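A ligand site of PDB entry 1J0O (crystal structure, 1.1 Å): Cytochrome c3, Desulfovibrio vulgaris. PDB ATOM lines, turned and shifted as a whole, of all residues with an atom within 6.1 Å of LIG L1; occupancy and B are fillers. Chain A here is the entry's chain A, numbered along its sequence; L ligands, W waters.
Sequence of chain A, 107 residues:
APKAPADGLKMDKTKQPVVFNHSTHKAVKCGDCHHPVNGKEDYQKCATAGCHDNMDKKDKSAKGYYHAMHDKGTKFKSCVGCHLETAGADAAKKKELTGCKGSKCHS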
ATOM      1  N   MET A  11      17.351 -20.340   2.735  1.00  0.00           N
ATOM      2  CA  MET A  11      18.210 -19.198   3.029  1.00  0.00           C
ATOM      3  C   MET A  11      18.816 -18.799   1.694  1.00  0.00           C
ATOM      4  O   MET A  11      19.560 -19.569   1.091  1.00  0.00           O
ATOM      5  CB  MET A  11      19.241 -19.605   4.045  1.00  0.00           C
ATOM      6  CG  MET A  11      18.611 -20.098   5.356  1.00  0.00           C
ATOM      7  SD  MET A  11      19.824 -20.611   6.563  1.00  0.00           S
ATOM      8  CE  MET A  11      20.418 -18.985   7.114  1.00  0.00           C
ATOM      9  N   ASP A  12      18.437 -17.615   1.225  1.00  0.00           N
ATOM     10  CA  ASP A  12      18.747 -17.271  -0.174  1.00  0.00           C
ATOM     11  C   ASP A  12      19.222 -15.851  -0.387  1.00  0.00           C
ATOM     12  O   ASP A  12      18.929 -15.216  -1.399  1.00  0.00           O
ATOM     13  CB  ASP A  12      17.481 -17.569  -1.012  1.00  0.00           C
ATOM     14  CG  ASP A  12      16.370 -16.602  -0.648  1.00  0.00           C
ATOM     15  OD1 ASP A  12      16.452 -15.785   0.300  1.00  0.00           O
ATOM     16  OD2 ASP A  12      15.340 -16.671  -1.361  1.00  0.00           O
ATOM     17  N   LYS A  13      20.051 -15.377   0.513  1.00  0.00           N
ATOM     18  CA  LYS A  13      20.676 -14.090   0.384  1.00  0.00           C
ATOM     19  C   LYS A  13      21.820 -14.087  -0.601  1.00  0.00           C
ATOM     20  O   LYS A  13      22.212 -13.023  -1.013  1.00  0.00           O
ATOM     21  CB  LYS A  13      21.187 -13.585   1.764  1.00  0.00           C
ATOM     22  CG  LYS A  13      20.065 -13.333   2.748  1.00  0.00           C
ATOM     23  CD  LYS A  13      19.341 -12.037   2.341  1.00  0.00           C
ATOM     24  CE  LYS A  13      17.880 -11.934   2.734  1.00  0.00           C
ATOM     25  NZ  LYS A  13      17.557 -10.508   2.496  1.00  0.00           N
ATOM     26  N   THR A  14      22.331 -15.255  -0.954  1.00  0.00           N
ATOM     27  CA  THR A  14      23.488 -15.424  -1.777  1.00  0.00           C
ATOM     28  C   THR A  14      23.198 -16.301  -2.990  1.00  0.00           C
ATOM     29  O   THR A  14      22.118 -16.898  -3.132  1.00  0.00           O
ATOM     30  CB  THR A  14      24.637 -16.047  -0.976  1.00  0.00           C
ATOM     31  OG1 THR A  14      24.457 -17.447  -0.810  1.00  0.00           O
ATOM     32  CG2 THR A  14      24.805 -15.483   0.424  1.00  0.00           C
ATOM     33  N   LYS A  15      24.193 -16.451  -3.865  1.00  0.00           N
ATOM     34  CA  LYS A  15      24.123 -17.355  -5.026  1.00  0.00           C
ATOM     35  C   LYS A  15      24.378 -18.823  -4.678  1.00  0.00           C
ATOM     36  O   LYS A  15      24.339 -19.697  -5.539  1.00  0.00           O
ATOM     37  CB  LYS A  15      25.059 -16.918  -6.155  1.00  0.00           C
ATOM     38  CG  LYS A  15      24.600 -15.544  -6.695  1.00  0.00           C
ATOM     39  CD  LYS A  15      25.259 -15.250  -8.014  1.00  0.00           C
ATOM     40  CE  LYS A  15      24.909 -13.864  -8.503  1.00  0.00           C
ATOM     41  NZ  LYS A  15      25.795 -13.504  -9.609  1.00  0.00           N
ATOM     42  N   GLN A  16      24.667 -19.213  -3.489  1.00  0.00           N
ATOM     43  CA  GLN A  16      24.731 -20.500  -2.856  1.00  0.00           C
ATOM     44  C   GLN A  16      23.664 -20.733  -1.795  1.00  0.00           C
ATOM     45  O   GLN A  16      23.981 -20.925  -0.617  1.00  0.00           O
ATOM     46  CB  GLN A  16      26.125 -20.711  -2.299  1.00  0.00           C
ATOM     47  CG  GLN A  16      27.206 -20.511  -3.308  1.00  0.00           C
ATOM     48  CD  GLN A  16      27.298 -21.583  -4.388  1.00  0.00           C
ATOM     49  OE1 GLN A  16      26.604 -22.612  -4.389  1.00  0.00           O
ATOM     50  NE2 GLN A  16      28.193 -21.300  -5.319  1.00  0.00           N
ATOM     51  N   PRO A  17      22.384 -20.723  -2.156  1.00  0.00           N
ATOM     52  CA  PRO A  17      21.327 -20.870  -1.158  1.00  0.00           C
ATOM     53  C   PRO A  17      21.325 -22.225  -0.489  1.00  0.00           C
ATOM     54  O   PRO A  17      21.759 -23.204  -1.052  1.00  0.00           O
ATOM     55  CB  PRO A  17      20.029 -20.776  -1.958  1.00  0.00           C
ATOM     56  CG  PRO A  17      20.429 -20.969  -3.393  1.00  0.00           C
ATOM     57  CD  PRO A  17      21.829 -20.565  -3.536  1.00  0.00           C
ATOM     58  N   VAL A  18      20.800 -22.252   0.732  1.00  0.00           N
ATOM     59  CA  VAL A  18      20.882 -23.446   1.572  1.00  0.00           C
ATOM     60  C   VAL A  18      19.506 -23.635   2.212  1.00  0.00           C
ATOM     61  O   VAL A  18      18.889 -22.645   2.719  1.00  0.00           O
ATOM     62  CB  VAL A  18      21.973 -23.277   2.655  1.00  0.00           C
ATOM     63  CG1 VAL A  18      21.903 -24.363   3.743  1.00  0.00           C
ATOM     64  CG2 VAL A  18      23.343 -23.193   2.050  1.00  0.00           C
ATOM     65  N   MET A  55      27.142  -8.597   3.145  1.00  0.00           N
ATOM     66  CA  MET A  55      27.265  -9.650   2.191  1.00  0.00           C
ATOM     67  C   MET A  55      28.650  -9.813   1.559  1.00  0.00           C
ATOM     68  O   MET A  55      28.809 -10.543   0.610  1.00  0.00           O
ATOM     69  CB  MET A  55      26.186  -9.486   1.136  1.00  0.00           C
ATOM     70  CG  MET A  55      24.748  -9.660   1.630  1.00  0.00           C
ATOM     71  SD  MET A  55      24.449 -11.336   2.256  1.00  0.00           S
ATOM     72  CE  MET A  55      23.447 -11.002   3.701  1.00  0.00           C
ATOM     73  N   ASP A  56      29.628  -9.128   2.169  1.00  0.00           N
ATOM     74  CA  ASP A  56      31.048  -9.387   1.876  1.00  0.00           C
ATOM     75  C   ASP A  56      31.493 -10.641   2.620  1.00  0.00           C
ATOM     76  O   ASP A  56      31.635 -10.618   3.829  1.00  0.00           O
ATOM     77  CB  ASP A  56      31.846  -8.191   2.328  1.00  0.00           C
ATOM     78  CG  ASP A  56      33.324  -8.323   2.308  1.00  0.00           C
ATOM     79  OD1 ASP A  56      33.992  -7.474   2.914  1.00  0.00           O
ATOM     80  OD2 ASP A  56      33.757  -9.298   1.672  1.00  0.00           O
ATOM     81  N   LYS A  57      31.696 -11.724   1.882  1.00  0.00           N
ATOM     82  CA  LYS A  57      32.022 -13.016   2.458  1.00  0.00           C
ATOM     83  C   LYS A  57      33.401 -13.035   3.108  1.00  0.00           C
ATOM     84  O   LYS A  57      33.637 -14.039   3.799  1.00  0.00           O
ATOM     85  CB  LYS A  57      31.826 -14.127   1.461  1.00  0.00           C
ATOM     86  CG  LYS A  57      32.849 -14.227   0.338  1.00  0.00           C
ATOM     87  CD  LYS A  57      32.568 -15.361  -0.628  1.00  0.00           C
ATOM     88  CE  LYS A  57      33.436 -15.353  -1.833  1.00  0.00           C
ATOM     89  NZ  LYS A  57      33.192 -16.541  -2.743  1.00  0.00           N
ATOM     90  N   TYR A  65      27.610 -11.911   7.148  1.00  0.00           N
ATOM     91  CA  TYR A  65      26.700 -13.020   7.013  1.00  0.00           C
ATOM     92  C   TYR A  65      27.423 -14.316   6.779  1.00  0.00           C
ATOM     93  O   TYR A  65      27.103 -15.318   7.463  1.00  0.00           O
ATOM     94  CB  TYR A  65      25.706 -12.681   5.887  1.00  0.00           C
ATOM     95  CG  TYR A  65      24.660 -13.693   5.624  1.00  0.00           C
ATOM     96  CD1 TYR A  65      24.589 -14.452   4.442  1.00  0.00           C
ATOM     97  CD2 TYR A  65      23.619 -13.957   6.472  1.00  0.00           C
ATOM     98  CE1 TYR A  65      23.616 -15.348   4.181  1.00  0.00           C
ATOM     99  CE2 TYR A  65      22.636 -14.861   6.250  1.00  0.00           C
ATOM    100  CZ  TYR A  65      22.632 -15.587   5.083  1.00  0.00           C
ATOM    101  OH  TYR A  65      21.643 -16.495   4.849  1.00  0.00           O
ATOM    102  N   TYR A  66      28.361 -14.381   5.880  1.00  0.00           N
ATOM    103  CA  TYR A  66      29.123 -15.592   5.658  1.00  0.00           C
ATOM    104  C   TYR A  66      29.784 -16.009   6.957  1.00  0.00           C
ATOM    105  O   TYR A  66      29.770 -17.182   7.331  1.00  0.00           O
ATOM    106  CB  TYR A  66      30.181 -15.353   4.535  1.00  0.00           C
ATOM    107  CG  TYR A  66      31.034 -16.585   4.277  1.00  0.00           C
ATOM    108  CD1 TYR A  66      32.180 -16.889   5.036  1.00  0.00           C
ATOM    109  CD2 TYR A  66      30.686 -17.467   3.263  1.00  0.00           C
ATOM    110  CE1 TYR A  66      32.933 -18.007   4.805  1.00  0.00           C
ATOM    111  CE2 TYR A  66      31.430 -18.603   2.994  1.00  0.00           C
ATOM    112  CZ  TYR A  66      32.538 -18.852   3.794  1.00  0.00           C
ATOM    113  OH  TYR A  66      33.249 -19.984   3.482  1.00  0.00           O
ATOM    114  N   MET A  69      27.604 -17.805   9.436  1.00  0.00           N
ATOM    115  CA  MET A  69      27.179 -19.136   9.054  1.00  0.00           C
ATOM    116  C   MET A  69      28.333 -20.155   9.035  1.00  0.00           C
ATOM    117  O   MET A  69      28.035 -21.357   9.154  1.00  0.00           O
ATOM    118  CB  MET A  69      26.457 -19.161   7.696  1.00  0.00           C
ATOM    119  CG  MET A  69      25.293 -18.201   7.543  1.00  0.00           C
ATOM    120  SD  MET A  69      23.998 -18.484   8.760  1.00  0.00           S
ATOM    121  CE  MET A  69      23.402 -16.872   9.030  1.00  0.00           C
ATOM    122  N   HIS A  70      29.571 -19.702   8.905  1.00  0.00           N
ATOM    123  CA  HIS A  70      30.668 -20.611   8.626  1.00  0.00           C
ATOM    124  C   HIS A  70      31.803 -20.672   9.646  1.00  0.00           C
ATOM    125  O   HIS A  70      32.530 -21.641   9.641  1.00  0.00           O
ATOM    126  CB  HIS A  70      31.295 -20.317   7.273  1.00  0.00           C
ATOM    127  CG  HIS A  70      30.413 -20.516   6.101  1.00  0.00           C
ATOM    128  ND1 HIS A  70      29.540 -19.491   5.694  1.00  0.00           N
ATOM    129  CD2 HIS A  70      30.152 -21.491   5.205  1.00  0.00           C
ATOM    130  CE1 HIS A  70      28.877 -19.921   4.614  1.00  0.00           C
ATOM    131  NE2 HIS A  70      29.193 -21.154   4.283  1.00  0.00           N
ATOM    132  N   CYS A  79      26.566 -22.415  11.815  1.00  0.00           N
ATOM    133  CA  CYS A  79      26.154 -23.678  11.171  1.00  0.00           C
ATOM    134  C   CYS A  79      27.334 -24.623  11.083  1.00  0.00           C
ATOM    135  O   CYS A  79      27.283 -25.795  11.564  1.00  0.00           O
ATOM    136  CB  CYS A  79      25.578 -23.465   9.799  1.00  0.00           C
ATOM    137  SG  CYS A  79      24.406 -22.122   9.490  1.00  0.00           S
ATOM    138  N   VAL A  80      28.386 -24.155  10.451  1.00  0.00           N
ATOM    139  CA  VAL A  80      29.563 -25.046  10.235  1.00  0.00           C
ATOM    140  C   VAL A  80      30.239 -25.341  11.536  1.00  0.00           C
ATOM    141  O   VAL A  80      30.673 -26.476  11.769  1.00  0.00           O
ATOM    142  CB  VAL A  80      30.508 -24.442   9.211  1.00  0.00           C
ATOM    143  CG1 VAL A  80      31.702 -25.364   9.005  1.00  0.00           C
ATOM    144  CG2 VAL A  80      29.809 -24.240   7.885  1.00  0.00           C
ATOM    145  N   HIS A  83      28.292 -27.996  13.299  1.00  0.00           N
ATOM    146  CA  HIS A  83      28.422 -29.258  12.545  1.00  0.00           C
ATOM    147  C   HIS A  83      29.802 -29.871  12.642  1.00  0.00           C
ATOM    148  O   HIS A  83      29.920 -31.123  12.703  1.00  0.00           O
ATOM    149  CB  HIS A  83      28.084 -29.005  11.090  1.00  0.00           C
ATOM    150  CG  HIS A  83      26.635 -28.833  10.847  1.00  0.00           C
ATOM    151  ND1 HIS A  83      26.141 -28.921   9.580  1.00  0.00           N
ATOM    152  CD2 HIS A  83      25.559 -28.581  11.598  1.00  0.00           C
ATOM    153  CE1 HIS A  83      24.825 -28.695   9.672  1.00  0.00           C
ATOM    154  NE2 HIS A  83      24.367 -28.476  10.891  1.00  0.00           N
ATOM    155  N   GLU A  96      29.271 -34.825   4.927  1.00  0.00           N
ATOM    156  CA  GLU A  96      27.857 -34.578   4.864  1.00  0.00           C
ATOM    157  C   GLU A  96      27.459 -33.260   5.490  1.00  0.00           C
ATOM    158  O   GLU A  96      26.569 -32.541   5.001  1.00  0.00           O
ATOM    159  CB  GLU A  96      27.102 -35.704   5.539  1.00  0.00           C
ATOM    160  CG  GLU A  96      25.630 -35.719   5.504  1.00  0.00           C
ATOM    161  CD  GLU A  96      25.125 -36.907   6.357  1.00  0.00           C
ATOM    162  OE1 GLU A  96      24.237 -36.739   7.200  1.00  0.00           O
ATOM    163  OE2 GLU A  96      25.670 -38.018   6.133  1.00  0.00           O
ATOM    164  N   LEU A  97      28.079 -32.925   6.629  1.00  0.00           N
ATOM    165  CA  LEU A  97      27.666 -31.816   7.466  1.00  0.00           C
ATOM    166  C   LEU A  97      28.553 -30.587   7.346  1.00  0.00           C
ATOM    167  O   LEU A  97      28.086 -29.498   7.703  1.00  0.00           O
ATOM    168  CB  LEU A  97      27.620 -32.222   8.946  1.00  0.00           C
ATOM    169  CG  LEU A  97      26.701 -33.377   9.285  1.00  0.00           C
ATOM    170  CD1 LEU A  97      26.768 -33.650  10.777  1.00  0.00           C
ATOM    171  CD2 LEU A  97      25.245 -33.050   8.908  1.00  0.00           C
ATOM    172  N   THR A  98      29.779 -30.745   6.828  1.00  0.00           N
ATOM    173  CA  THR A  98      30.694 -29.597   6.753  1.00  0.00           C
ATOM    174  C   THR A  98      31.302 -29.435   5.361  1.00  0.00           C
ATOM    175  O   THR A  98      32.030 -28.431   5.216  1.00  0.00           O
ATOM    176  CB  THR A  98      31.797 -29.641   7.800  1.00  0.00           C
ATOM    177  OG1 THR A  98      32.828 -30.587   7.515  1.00  0.00           O
ATOM    178  CG2 THR A  98      31.241 -29.951   9.181  1.00  0.00           C
ATOM    179  N   GLY A  99      31.111 -30.297   4.414  1.00  0.00           N
ATOM    180  CA  GLY A  99      31.748 -30.143   3.116  1.00  0.00           C
ATOM    181  C   GLY A  99      31.272 -28.897   2.421  1.00  0.00           C
ATOM    182  O   GLY A  99      30.122 -28.471   2.487  1.00  0.00           O
ATOM    183  N   CYS A 100      32.198 -28.311   1.690  1.00  0.00           N
ATOM    184  CA  CYS A 100      31.918 -27.076   0.955  1.00  0.00           C
ATOM    185  C   CYS A 100      31.163 -27.378  -0.326  1.00  0.00           C
ATOM    186  O   CYS A 100      30.532 -26.509  -0.879  1.00  0.00           O
ATOM    187  CB  CYS A 100      33.175 -26.308   0.676  1.00  0.00           C
ATOM    188  SG  CYS A 100      34.247 -25.997   2.089  1.00  0.00           S
ATOM    189  N   LYS A 101      31.240 -28.591  -0.818  1.00  0.00           N
ATOM    190  CA  LYS A 101      30.414 -29.013  -1.922  1.00  0.00           C
ATOM    191  C   LYS A 101      30.046 -30.454  -1.671  1.00  0.00           C
ATOM    192  O   LYS A 101      30.758 -31.055  -0.867  1.00  0.00           O
ATOM    193  CB  LYS A 101      31.134 -28.869  -3.264  1.00  0.00           C
ATOM    194  CG  LYS A 101      32.426 -29.621  -3.318  1.00  0.00           C
ATOM    195  CD  LYS A 101      32.990 -29.423  -4.740  1.00  0.00           C
ATOM    196  CE  LYS A 101      33.667 -30.681  -5.281  1.00  0.00           C
ATOM    197  NZ  LYS A 101      32.673 -31.657  -5.808  1.00  0.00           N
ATOM    198  N   SER A 103      27.727 -31.607   0.104  1.00  0.00           N
ATOM    199  CA  SER A 103      27.253 -31.738   1.480  1.00  0.00           C
ATOM    200  C   SER A 103      25.759 -31.554   1.539  1.00  0.00           C
ATOM    201  O   SER A 103      25.092 -31.252   0.572  1.00  0.00           O
ATOM    202  CB  SER A 103      27.971 -30.783   2.395  1.00  0.00           C
ATOM    203  OG  SER A 103      27.651 -29.427   2.120  1.00  0.00           O
ATOM    204  N   LYS A 104      25.165 -31.649   2.733  1.00  0.00           N
ATOM    205  CA  LYS A 104      23.758 -31.420   2.908  1.00  0.00           C
ATOM    206  C   LYS A 104      23.436 -29.953   2.867  1.00  0.00           C
ATOM    207  O   LYS A 104      22.271 -29.556   2.697  1.00  0.00           O
ATOM    208  CB  LYS A 104      23.252 -32.070   4.218  1.00  0.00           C
ATOM    209  CG  LYS A 104      23.218 -33.579   4.114  1.00  0.00           C
ATOM    210  CD  LYS A 104      22.582 -34.345   5.237  1.00  0.00           C
ATOM    211  CE  LYS A 104      22.398 -35.796   4.861  1.00  0.00           C
ATOM    212  NZ  LYS A 104      21.393 -36.074   3.837  1.00  0.00           N
ATOM    213  N   CYS A 105      24.376 -29.039   2.984  1.00  0.00           N
ATOM    214  CA  CYS A 105      24.215 -27.629   2.788  1.00  0.00           C
ATOM    215  C   CYS A 105      24.369 -27.188   1.335  1.00  0.00           C
ATOM    216  O   CYS A 105      23.545 -26.475   0.824  1.00  0.00           O
ATOM    217  CB  CYS A 105      25.166 -26.806   3.651  1.00  0.00           C
ATOM    218  SG  CYS A 105      24.841 -27.129   5.398  1.00  0.00           S
ATOM    219  N   HIS A 106      25.439 -27.509   0.665  1.00  0.00           N
ATOM    220  CA  HIS A 106      25.785 -27.135  -0.678  1.00  0.00           C
ATOM    221  C   HIS A 106      25.955 -28.358  -1.544  1.00  0.00           C
ATOM    222  O   HIS A 106      26.820 -29.184  -1.310  1.00  0.00           O
ATOM    223  CB  HIS A 106      27.091 -26.350  -0.693  1.00  0.00           C
ATOM    224  CG  HIS A 106      27.151 -25.074   0.072  1.00  0.00           C
ATOM    225  ND1 HIS A 106      26.285 -24.040  -0.170  1.00  0.00           N
ATOM    226  CD2 HIS A 106      27.925 -24.620   1.069  1.00  0.00           C
ATOM    227  CE1 HIS A 106      26.598 -23.045   0.670  1.00  0.00           C
ATOM    228  NE2 HIS A 106      27.611 -23.338   1.472  1.00  0.00           N
HETATM  229  C1  LIG L   1      26.704 -19.546   1.667  1.00  0.00           C
HETATM  230  C2  LIG L   1      31.052 -21.429   0.850  1.00  0.00           C
HETATM  231  C3  LIG L   1      30.066 -24.987   3.857  1.00  0.00           C
HETATM  232  C4  LIG L   1      25.885 -22.891   4.984  1.00  0.00           C
HETATM  233  C5  LIG L   1      27.915 -19.765   1.062  1.00  0.00           C
HETATM  234  C6  LIG L   1      28.547 -19.034   0.032  1.00  0.00           C
HETATM  235  C7  LIG L   1      29.765 -19.568  -0.210  1.00  0.00           C
HETATM  236  C8  LIG L   1      29.936 -20.688   0.671  1.00  0.00           C
HETATM  237  C9  LIG L   1      30.779 -19.127  -1.238  1.00  0.00           C
HETATM  238  C10 LIG L   1      27.984 -17.794  -0.636  1.00  0.00           C
HETATM  239  C11 LIG L   1      28.614 -16.527  -0.046  1.00  0.00           C
HETATM  240  C12 LIG L   1      28.277 -15.255  -0.822  1.00  0.00           C
HETATM  241  O1  LIG L   1      28.376 -15.298  -2.073  1.00  0.00           O
HETATM  242  O2  LIG L   1      27.853 -14.275  -0.216  1.00  0.00           O
HETATM  243  C13 LIG L   1      31.254 -22.459   1.744  1.00  0.00           C
HETATM  244  C14 LIG L   1      32.496 -23.187   1.932  1.00  0.00           C
HETATM  245  C15 LIG L   1      32.208 -24.240   2.747  1.00  0.00           C
HETATM  246  C16 LIG L   1      30.816 -24.145   3.087  1.00  0.00           C
HETATM  247  C17 LIG L   1      33.809 -22.760   1.304  1.00  0.00           C
HETATM  248  C18 LIG L   1      33.106 -25.217   3.322  1.00  0.00           C
HETATM  249  C19 LIG L   1      33.987 -24.695   4.401  1.00  0.00           C
HETATM  250  C20 LIG L   1      28.771 -24.820   4.323  1.00  0.00           C
HETATM  251  C21 LIG L   1      28.012 -25.770   5.075  1.00  0.00           C
HETATM  252  C22 LIG L   1      26.802 -25.159   5.484  1.00  0.00           C
HETATM  253  C23 LIG L   1      26.850 -23.856   4.850  1.00  0.00           C
HETATM  254  C24 LIG L   1      28.508 -27.194   5.394  1.00  0.00           C
HETATM  255  C25 LIG L   1      25.675 -25.751   6.239  1.00  0.00           C
HETATM  256  C26 LIG L   1      26.082 -26.213   7.565  1.00  0.00           C
HETATM  257  C27 LIG L   1      25.770 -21.729   4.260  1.00  0.00           C
HETATM  258  C28 LIG L   1      24.707 -20.771   4.377  1.00  0.00           C
HETATM  259  C29 LIG L   1      24.895 -19.858   3.410  1.00  0.00           C
HETATM  260  C30 LIG L   1      26.101 -20.220   2.698  1.00  0.00           C
HETATM  261  C31 LIG L   1      23.599 -20.857   5.396  1.00  0.00           C
HETATM  262  C32 LIG L   1      24.021 -18.729   3.053  1.00  0.00           C
HETATM  263  C33 LIG L   1      22.876 -19.111   2.135  1.00  0.00           C
HETATM  264  C34 LIG L   1      22.099 -17.933   1.554  1.00  0.00           C
HETATM  265  O3  LIG L   1      21.496 -17.179   2.315  1.00  0.00           O
HETATM  266  O4  LIG L   1      22.159 -17.755   0.308  1.00  0.00           O
HETATM  267  N1  LIG L   1      28.778 -20.744   1.443  1.00  0.00           N
HETATM  268  N2  LIG L   1      30.261 -23.019   2.483  1.00  0.00           N
HETATM  269  N3  LIG L   1      28.020 -23.707   4.157  1.00  0.00           N
HETATM  270  N4  LIG L   1      26.601 -21.338   3.260  1.00  0.00           N
HETATM  271 FE1  LIG L   1      28.414 -22.227   2.842  1.00  0.00          FE
HETATM  272  C1  LG2 L   2      21.822 -31.410  10.585  1.00  0.00           C
HETATM  273  C2  LG2 L   2      21.882 -27.213   8.243  1.00  0.00           C
HETATM  274  C3  LG2 L   2      23.062 -24.993  12.271  1.00  0.00           C
HETATM  275  C4  LG2 L   2      23.361 -29.183  14.565  1.00  0.00           C
HETATM  276  C5  LG2 L   2      21.695 -30.507   9.551  1.00  0.00           C
HETATM  277  C6  LG2 L   2      21.442 -30.762   8.166  1.00  0.00           C
HETATM  278  C7  LG2 L   2      21.493 -29.602   7.510  1.00  0.00           C
HETATM  279  C8  LG2 L   2      21.761 -28.557   8.486  1.00  0.00           C
HETATM  280  C9  LG2 L   2      21.259 -29.324   6.047  1.00  0.00           C
HETATM  281  C10 LG2 L   2      21.159 -32.145   7.587  1.00  0.00           C
HETATM  282  C11 LG2 L   2      19.727 -32.578   7.900  1.00  0.00           C
HETATM  283  C12 LG2 L   2      18.759 -31.664   7.118  1.00  0.00           C
HETATM  284  O1  LG2 L   2      18.705 -31.884   5.880  1.00  0.00           O
HETATM  285  O2  LG2 L   2      18.001 -30.939   7.799  1.00  0.00           O
HETATM  286  C13 LG2 L   2      22.186 -26.219   9.104  1.00  0.00           C
HETATM  287  C14 LG2 L   2      22.334 -24.818   8.798  1.00  0.00           C
HETATM  288  C15 LG2 L   2      22.611 -24.166   9.958  1.00  0.00           C
HETATM  289  C16 LG2 L   2      22.666 -25.184  10.991  1.00  0.00           C
HETATM  290  C17 LG2 L   2      22.195 -24.248   7.362  1.00  0.00           C
HETATM  291  C18 LG2 L   2      22.842 -22.725  10.194  1.00  0.00           C
HETATM  292  C19 LG2 L   2      21.768 -21.785   9.738  1.00  0.00           C
HETATM  293  C20 LG2 L   2      23.266 -25.916  13.269  1.00  0.00           C
HETATM  294  C21 LG2 L   2      23.691 -25.589  14.623  1.00  0.00           C
HETATM  295  C22 LG2 L   2      23.871 -26.787  15.304  1.00  0.00           C
HETATM  296  C23 LG2 L   2      23.449 -27.806  14.344  1.00  0.00           C
HETATM  297  C24 LG2 L   2      24.046 -24.159  15.039  1.00  0.00           C
HETATM  298  C25 LG2 L   2      24.409 -27.067  16.617  1.00  0.00           C
HETATM  299  C26 LG2 L   2      24.199 -26.121  17.645  1.00  0.00           C
HETATM  300  C27 LG2 L   2      22.911 -30.156  13.717  1.00  0.00           C
HETATM  301  C28 LG2 L   2      22.734 -31.571  14.049  1.00  0.00           C
HETATM  302  C29 LG2 L   2      22.293 -32.188  12.939  1.00  0.00           C
HETATM  303  C30 LG2 L   2      22.250 -31.202  11.895  1.00  0.00           C
HETATM  304  C31 LG2 L   2      22.985 -32.144  15.434  1.00  0.00           C
HETATM  305  C32 LG2 L   2      22.036 -33.645  12.696  1.00  0.00           C
HETATM  306  C33 LG2 L   2      23.294 -34.323  12.220  1.00  0.00           C
HETATM  307  C34 LG2 L   2      23.131 -35.673  11.616  1.00  0.00           C
HETATM  308  O3  LG2 L   2      24.121 -36.396  11.637  1.00  0.00           O
HETATM  309  O4  LG2 L   2      22.023 -36.174  11.327  1.00  0.00           O
HETATM  310  N1  LG2 L   2      21.839 -29.145   9.721  1.00  0.00           N
HETATM  311  N2  LG2 L   2      22.453 -26.415  10.396  1.00  0.00           N
HETATM  312  N3  LG2 L   2      23.155 -27.232  13.149  1.00  0.00           N
HETATM  313  N4  LG2 L   2      22.562 -29.986  12.423  1.00  0.00           N
HETATM  314 FE1  LG2 L   2      22.513 -28.197  11.422  1.00  0.00          FE
HETATM  315  O   HOH W   1      30.335 -16.388  -3.479  1.00  0.00           O
HETATM  316  O   HOH W   2      27.312 -13.442   2.254  1.00  0.00           O
HETATM  317  O   HOH W   3      26.660 -16.609   3.187  1.00  0.00           O
HETATM  318  O   HOH W   4      27.052 -11.933  -1.037  1.00  0.00           O
HETATM  319  O   HOH W   5      26.488 -14.629  -3.833  1.00  0.00           O
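C25 of LIG L1 is covalently linked to SG of Cys 105 (1.8 Å).
SG of Cys 100 is covalently linked to C18 of LIG L1, at 1.9 Å.
An iron atom (FE1) of LIG L1 is bound by a ring nitrogen (NE2) of His 106, 1.9 Å away.
NE2 of His 70 is bound to FE1 of LIG L1 (2.0 Å).
O4 of LIG L1 is in hydrogen-bond range of N of Thr 14 (2.8 Å).
An oxygen (O4) of LIG L1 is in hydrogen-bond range of the side-chain hydroxyl of Thr 14, at 2.6 Å.
An oxygen (O3) of LIG L1 lies within hydrogen-bond range of the side-chain hydroxyl of Tyr 65, at 2.6 Å.
N of Lys 13 sits at hydrogen-bond distance from O3 of LIG L1, 2.9 Å away.
N of Asp 12 sits at hydrogen-bond distance from O3 of LIG L1, 3.3 Å away.
NE2 of His 83 binds FE1 of LG2 L2, at 1.9 Å.
The side-chain sulfur (SG) of Cys 79 is bonded to a carbon (C18) of LG2 L2 (1.8 Å).
The backbone NH of Cys 105 sits close to the side-chain hydroxyl of Ser 103 (3.4 Å).
N of His 106 sits at hydrogen-bond distance from OG of Ser 103 (3.3 Å).
The backbone carbonyl oxygen (O) of Tyr 66 sits at hydrogen-bond distance from a ring nitrogen (ND1) of His 70 (2.8 Å).
The side-chain hydroxyl (OG1) of Thr 14 is in hydrogen-bond range of the backbone NH (N) of Gln 16, at 3.2 Å.
O of Leu 97 is in hydrogen-bond range of ND1 of His 83, 2.8 Å away.
The backbone carbonyl oxygen (O) of Gly 99 is in hydrogen-bond range of the side-chain hydroxyl (OG) of Ser 103, 2.7 Å away.
N of Cys 79 lies within hydrogen-bond range of O of Met 69, 3.2 Å away.
The backbone NH of Val 80 lies within hydrogen-bond range of the backbone carbonyl oxygen of Met 69 (3.1 Å).
Water W4 lies within hydrogen-bond range of an oxygen (O2) of LIG L1 (2.6 Å) and the backbone carbonyl oxygen (O) of Met 55 (2.8 Å).
Water W1 lies within hydrogen-bond range of O1 of LIG L1 and NZ of Lys 57.
Water W2 lies within hydrogen-bond range of an oxygen (O2) of LIG L1 (2.7 Å) and the side-chain sulfur of Met 55 (3.6 Å).
Water W5 lies within hydrogen-bond range of an oxygen (O1) of LIG L1 (2.7 Å) and the backbone NH of Lys 15 (2.9 Å).
The backbone carbonyl oxygen (O) of Met 11 lies close to an oxygen (O4) of LIG L1 (3.3 Å).
Gln 16 touches LIG L1 (O to C33, 3.5 Å).
Pro 17 touches LIG L1 (CA to O4, 3.5 Å).
Val 18 touches LIG L1 (CG2 to C27, 3.6 Å).
Met 55 touches LIG L1 (O to O2, 3.9 Å).
Lys 57 touches LIG L1 (NZ to C9, 3.8 Å).
CE2 of Tyr 66 touches C8 of LIG L1, at 3.5 Å.
Met 69 touches LIG L1 (CG to C31, 3.8 Å).
CB of Cys 79 touches C26 of LIG L1, at 3.6 Å.
CG2 of Val 80 touches C21 of LIG L1, at 3.7 Å.
ND1 of His 83 touches C26 of LIG L1, at 3.4 Å.
Leu 97 touches LIG L1 (O to C24, 3.3 Å).
Thr 98 touches LIG L1.
O of Gly 99 touches C24 of LIG L1 (3.6 Å).
Hydrophobic or aromatic side chains that line LIG L1: Met 11, Val 18, Tyr 65, Tyr 66, Met 69, His 70, Val 80, His 83 and His 106.
Within 4 Å of LIG L1: Met 11, Asp 12, Lys 13, Thr 14, Gln 16, Pro 17, Val 18, Met 55, Lys 57, Tyr 65, Tyr 66, Met 69, His 70, Cys 79, Val 80, His 83, Leu 97, Thr 98, Gly 99, Cys 100, Cys 105 and His 106.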
